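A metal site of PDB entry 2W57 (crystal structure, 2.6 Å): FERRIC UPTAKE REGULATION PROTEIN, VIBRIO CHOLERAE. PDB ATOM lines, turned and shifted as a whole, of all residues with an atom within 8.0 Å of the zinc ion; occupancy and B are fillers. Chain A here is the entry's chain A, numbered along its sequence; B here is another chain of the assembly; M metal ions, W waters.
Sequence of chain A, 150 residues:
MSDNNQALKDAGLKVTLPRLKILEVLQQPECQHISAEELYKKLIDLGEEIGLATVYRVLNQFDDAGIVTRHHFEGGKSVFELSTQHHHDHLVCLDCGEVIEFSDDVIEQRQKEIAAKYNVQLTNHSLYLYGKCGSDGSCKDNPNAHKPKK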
ATOM      1  N   HIS A  87     -11.317   0.333  15.443  1.00  0.00           N
ATOM      2  CA  HIS A  87     -12.641  -0.216  15.200  1.00  0.00           C
ATOM      3  C   HIS A  87     -13.350   0.464  14.045  1.00  0.00           C
ATOM      4  O   HIS A  87     -13.374   1.696  13.964  1.00  0.00           O
ATOM      5  CB  HIS A  87     -13.485  -0.077  16.470  1.00  0.00           C
ATOM      6  CG  HIS A  87     -14.914  -0.475  16.284  1.00  0.00           C
ATOM      7  ND1 HIS A  87     -15.340  -1.791  16.416  1.00  0.00           N
ATOM      8  CD2 HIS A  87     -16.012   0.255  15.992  1.00  0.00           C
ATOM      9  CE1 HIS A  87     -16.646  -1.846  16.198  1.00  0.00           C
ATOM     10  NE2 HIS A  87     -17.075  -0.614  15.936  1.00  0.00           N
ATOM     11  N   HIS A  88     -13.934  -0.335  13.147  1.00  0.00           N
ATOM     12  CA  HIS A  88     -14.897   0.181  12.185  1.00  0.00           C
ATOM     13  C   HIS A  88     -16.053  -0.805  11.900  1.00  0.00           C
ATOM     14  O   HIS A  88     -16.037  -1.976  12.307  1.00  0.00           O
ATOM     15  CB  HIS A  88     -14.196   0.651  10.893  1.00  0.00           C
ATOM     16  CG  HIS A  88     -13.422  -0.420  10.191  1.00  0.00           C
ATOM     17  ND1 HIS A  88     -12.200  -0.874  10.634  1.00  0.00           N
ATOM     18  CD2 HIS A  88     -13.687  -1.115   9.060  1.00  0.00           C
ATOM     19  CE1 HIS A  88     -11.747  -1.805   9.814  1.00  0.00           C
ATOM     20  NE2 HIS A  88     -12.632  -1.975   8.847  1.00  0.00           N
ATOM     21  N   ASP A  89     -17.095  -0.289  11.248  1.00  0.00           N
ATOM     22  CA  ASP A  89     -18.203  -1.093  10.766  1.00  0.00           C
ATOM     23  C   ASP A  89     -18.239  -0.967   9.260  1.00  0.00           C
ATOM     24  O   ASP A  89     -17.405  -0.255   8.689  1.00  0.00           O
ATOM     25  CB  ASP A  89     -19.500  -0.633  11.419  1.00  0.00           C
ATOM     26  CG  ASP A  89     -19.454  -0.802  12.899  1.00  0.00           C
ATOM     27  OD1 ASP A  89     -19.151  -1.928  13.345  1.00  0.00           O
ATOM     28  OD2 ASP A  89     -19.687   0.184  13.625  1.00  0.00           O
ATOM     29  N   HIS A  90     -19.170  -1.648   8.611  1.00  0.00           N
ATOM     30  CA  HIS A  90     -19.076  -1.803   7.171  1.00  0.00           C
ATOM     31  C   HIS A  90     -20.359  -1.501   6.442  1.00  0.00           C
ATOM     32  O   HIS A  90     -21.437  -1.936   6.838  1.00  0.00           O
ATOM     33  CB  HIS A  90     -18.565  -3.190   6.793  1.00  0.00           C
ATOM     34  CG  HIS A  90     -17.331  -3.607   7.535  1.00  0.00           C
ATOM     35  ND1 HIS A  90     -17.376  -4.093   8.831  1.00  0.00           N
ATOM     36  CD2 HIS A  90     -16.024  -3.608   7.182  1.00  0.00           C
ATOM     37  CE1 HIS A  90     -16.144  -4.373   9.235  1.00  0.00           C
ATOM     38  NE2 HIS A  90     -15.306  -4.092   8.252  1.00  0.00           N
ATOM     39  N   PHE A 102     -16.992   2.792   8.339  1.00  0.00           N
ATOM     40  CA  PHE A 102     -17.473   3.946   9.104  1.00  0.00           C
ATOM     41  C   PHE A 102     -17.433   3.644  10.593  1.00  0.00           C
ATOM     42  O   PHE A 102     -17.370   2.489  11.007  1.00  0.00           O
ATOM     43  CB  PHE A 102     -18.885   4.363   8.650  1.00  0.00           C
ATOM     44  CG  PHE A 102     -19.972   3.385   9.035  1.00  0.00           C
ATOM     45  CD1 PHE A 102     -20.265   2.293   8.209  1.00  0.00           C
ATOM     46  CD2 PHE A 102     -20.703   3.563  10.203  1.00  0.00           C
ATOM     47  CE1 PHE A 102     -21.269   1.389   8.549  1.00  0.00           C
ATOM     48  CE2 PHE A 102     -21.707   2.650  10.555  1.00  0.00           C
ATOM     49  CZ  PHE A 102     -21.987   1.571   9.720  1.00  0.00           C
ATOM     50  N   SER A 103     -17.487   4.704  11.398  1.00  0.00           N
ATOM     51  CA  SER A 103     -17.563   4.580  12.837  1.00  0.00           C
ATOM     52  C   SER A 103     -18.375   5.747  13.416  1.00  0.00           C
ATOM     53  O   SER A 103     -17.829   6.797  13.730  1.00  0.00           O
ATOM     54  CB  SER A 103     -16.155   4.524  13.453  1.00  0.00           C
ATOM     55  OG  SER A 103     -16.229   4.259  14.849  1.00  0.00           O
ATOM     56  N   ASP A 104     -19.676   5.539  13.541  1.00  0.00           N
ATOM     57  CA  ASP A 104     -20.588   6.557  14.010  1.00  0.00           C
ATOM     58  C   ASP A 104     -20.668   6.569  15.534  1.00  0.00           C
ATOM     59  O   ASP A 104     -20.864   5.522  16.155  1.00  0.00           O
ATOM     60  CB  ASP A 104     -21.972   6.285  13.426  1.00  0.00           C
ATOM     61  CG  ASP A 104     -22.938   7.427  13.628  1.00  0.00           C
ATOM     62  OD1 ASP A 104     -22.702   8.517  13.043  1.00  0.00           O
ATOM     63  OD2 ASP A 104     -23.928   7.246  14.367  1.00  0.00           O
ATOM     64  N   ILE A 107     -24.473   5.753  16.940  1.00  0.00           N
ATOM     65  CA  ILE A 107     -24.669   4.303  16.896  1.00  0.00           C
ATOM     66  C   ILE A 107     -23.838   3.624  17.984  1.00  0.00           C
ATOM     67  O   ILE A 107     -24.385   2.840  18.773  1.00  0.00           O
ATOM     68  CB  ILE A 107     -24.363   3.707  15.512  1.00  0.00           C
ATOM     69  CG1 ILE A 107     -25.382   4.211  14.483  1.00  0.00           C
ATOM     70  CG2 ILE A 107     -24.350   2.165  15.565  1.00  0.00           C
ATOM     71  CD1 ILE A 107     -25.006   3.936  13.064  1.00  0.00           C
ATOM     72  N   GLU A 108     -22.544   3.928  18.057  1.00  0.00           N
ATOM     73  CA  GLU A 108     -21.714   3.332  19.094  1.00  0.00           C
ATOM     74  C   GLU A 108     -22.340   3.508  20.475  1.00  0.00           C
ATOM     75  O   GLU A 108     -22.452   2.537  21.219  1.00  0.00           O
ATOM     76  CB  GLU A 108     -20.270   3.878  19.072  1.00  0.00           C
ATOM     77  CG  GLU A 108     -19.418   3.485  17.850  1.00  0.00           C
ATOM     78  CD  GLU A 108     -19.500   1.999  17.477  1.00  0.00           C
ATOM     79  OE1 GLU A 108     -19.584   1.131  18.362  1.00  0.00           O
ATOM     80  OE2 GLU A 108     -19.480   1.709  16.262  1.00  0.00           O
ATOM     81  N   GLN A 111     -25.846   1.409  21.104  1.00  0.00           N
ATOM     82  CA  GLN A 111     -25.560  -0.011  21.380  1.00  0.00           C
ATOM     83  C   GLN A 111     -25.343  -0.278  22.876  1.00  0.00           C
ATOM     84  O   GLN A 111     -25.914  -1.231  23.423  1.00  0.00           O
ATOM     85  CB  GLN A 111     -24.346  -0.472  20.548  1.00  0.00           C
ATOM     86  CG  GLN A 111     -24.545  -0.367  19.026  1.00  0.00           C
ATOM     87  CD  GLN A 111     -23.320  -0.767  18.209  1.00  0.00           C
ATOM     88  OE1 GLN A 111     -22.233  -0.936  18.747  1.00  0.00           O
ATOM     89  NE2 GLN A 111     -23.491  -0.889  16.897  1.00  0.00           N
ATOM     90  N   ASN A 124     -18.687  -6.995  22.573  1.00  0.00           N
ATOM     91  CA  ASN A 124     -18.348  -6.840  21.161  1.00  0.00           C
ATOM     92  C   ASN A 124     -19.632  -6.696  20.356  1.00  0.00           C
ATOM     93  O   ASN A 124     -20.717  -7.019  20.845  1.00  0.00           O
ATOM     94  CB  ASN A 124     -17.535  -8.054  20.690  1.00  0.00           C
ATOM     95  CG  ASN A 124     -16.896  -7.851  19.321  1.00  0.00           C
ATOM     96  OD1 ASN A 124     -16.881  -6.742  18.790  1.00  0.00           O
ATOM     97  ND2 ASN A 124     -16.376  -8.935  18.744  1.00  0.00           N
ATOM     98  N   HIS A 125     -19.511  -6.189  19.126  1.00  0.00           N
ATOM     99  CA  HIS A 125     -20.640  -6.116  18.195  1.00  0.00           C
ATOM    100  C   HIS A 125     -20.162  -6.275  16.758  1.00  0.00           C
ATOM    101  O   HIS A 125     -18.964  -6.252  16.484  1.00  0.00           O
ATOM    102  CB  HIS A 125     -21.414  -4.808  18.386  1.00  0.00           C
ATOM    103  CG  HIS A 125     -20.687  -3.588  17.902  1.00  0.00           C
ATOM    104  ND1 HIS A 125     -19.769  -2.924  18.683  1.00  0.00           N
ATOM    105  CD2 HIS A 125     -20.766  -2.900  16.741  1.00  0.00           C
ATOM    106  CE1 HIS A 125     -19.298  -1.882  18.022  1.00  0.00           C
ATOM    107  NE2 HIS A 125     -19.897  -1.839  16.838  1.00  0.00           N
ATOM    108  N   SER A 126     -21.088  -6.461  15.822  1.00  0.00           N
ATOM    109  CA  SER A 126     -20.752  -6.350  14.410  1.00  0.00           C
ATOM    110  C   SER A 126     -21.927  -5.756  13.670  1.00  0.00           C
ATOM    111  O   SER A 126     -23.071  -6.123  13.927  1.00  0.00           O
ATOM    112  CB  SER A 126     -20.329  -7.699  13.802  1.00  0.00           C
ATOM    113  OG  SER A 126     -21.361  -8.668  13.903  1.00  0.00           O
ATOM    114  N   LEU A 127     -21.635  -4.828  12.760  1.00  0.00           N
ATOM    115  CA  LEU A 127     -22.688  -4.117  12.012  1.00  0.00           C
ATOM    116  C   LEU A 127     -22.348  -4.049  10.537  1.00  0.00           C
ATOM    117  O   LEU A 127     -21.277  -3.578  10.162  1.00  0.00           O
ATOM    118  CB  LEU A 127     -22.926  -2.709  12.602  1.00  0.00           C
ATOM    119  CG  LEU A 127     -23.726  -1.655  11.846  1.00  0.00           C
ATOM    120  CD1 LEU A 127     -25.180  -2.053  11.696  1.00  0.00           C
ATOM    121  CD2 LEU A 127     -23.619  -0.303  12.550  1.00  0.00           C
ATOM    122  N   LEU B 127     -27.285  -6.340  12.595  1.00  0.00           N
ATOM    123  CA  LEU B 127     -26.676  -5.759  13.792  1.00  0.00           C
ATOM    124  C   LEU B 127     -26.679  -6.776  14.924  1.00  0.00           C
ATOM    125  O   LEU B 127     -27.730  -7.084  15.500  1.00  0.00           O
ATOM    126  CB  LEU B 127     -27.399  -4.476  14.194  1.00  0.00           C
ATOM    127  CG  LEU B 127     -27.162  -3.763  15.541  1.00  0.00           C
ATOM    128  CD1 LEU B 127     -25.686  -3.452  15.775  1.00  0.00           C
ATOM    129  CD2 LEU B 127     -28.003  -2.485  15.612  1.00  0.00           C
ATOM    130  N   LEU B 129     -25.195  -7.532  18.567  1.00  0.00           N
ATOM    131  CA  LEU B 129     -24.541  -7.066  19.762  1.00  0.00           C
ATOM    132  C   LEU B 129     -24.254  -8.310  20.597  1.00  0.00           C
ATOM    133  O   LEU B 129     -25.150  -9.122  20.835  1.00  0.00           O
ATOM    134  CB  LEU B 129     -25.446  -6.084  20.533  1.00  0.00           C
ATOM    135  CG  LEU B 129     -25.913  -4.789  19.852  1.00  0.00           C
ATOM    136  CD1 LEU B 129     -26.787  -3.927  20.772  1.00  0.00           C
ATOM    137  CD2 LEU B 129     -24.745  -3.968  19.302  1.00  0.00           C
HETATM  138 ZN    ZN M   1     -19.265  -0.218  15.488  1.00  0.00          ZN
HETATM  139  O   HOH W   1     -20.871   2.565  14.149  1.00  0.00           O
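The side-chain carboxylate (OE1) of Glu 108 lies close to the side-chain amide oxygen (OE1) of Gln 111 (3.4 Å). A ring nitrogen (ND1) of His 125 is in hydrogen-bond range of the side-chain amide oxygen (OE1) of Gln 111, 3.2 Å away. O of Phe 102 lies within hydrogen-bond range of N of Asp 89 (2.8 Å).
Within 4 Å of the zinc ion: His 87, Asp 89, Glu 108 and His 125. The nearest printed residue that does not touch the zinc ion is Gln 111 (4.5 Å).
OD2 of Asp 89 is bound to the zinc ion. The side-chain carboxylate (OE2) of Glu 108 is bound to the zinc ion (2.1 Å). The zinc ion is bound by NE2 of His 125, at 2.2 Å. NE2 of His 87 binds the zinc ion (2.3 Å). The zinc ion has four donor atoms within binding distance. Slightly farther from the zinc ion lies OD1 of Asp 89 (2.7 Å).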
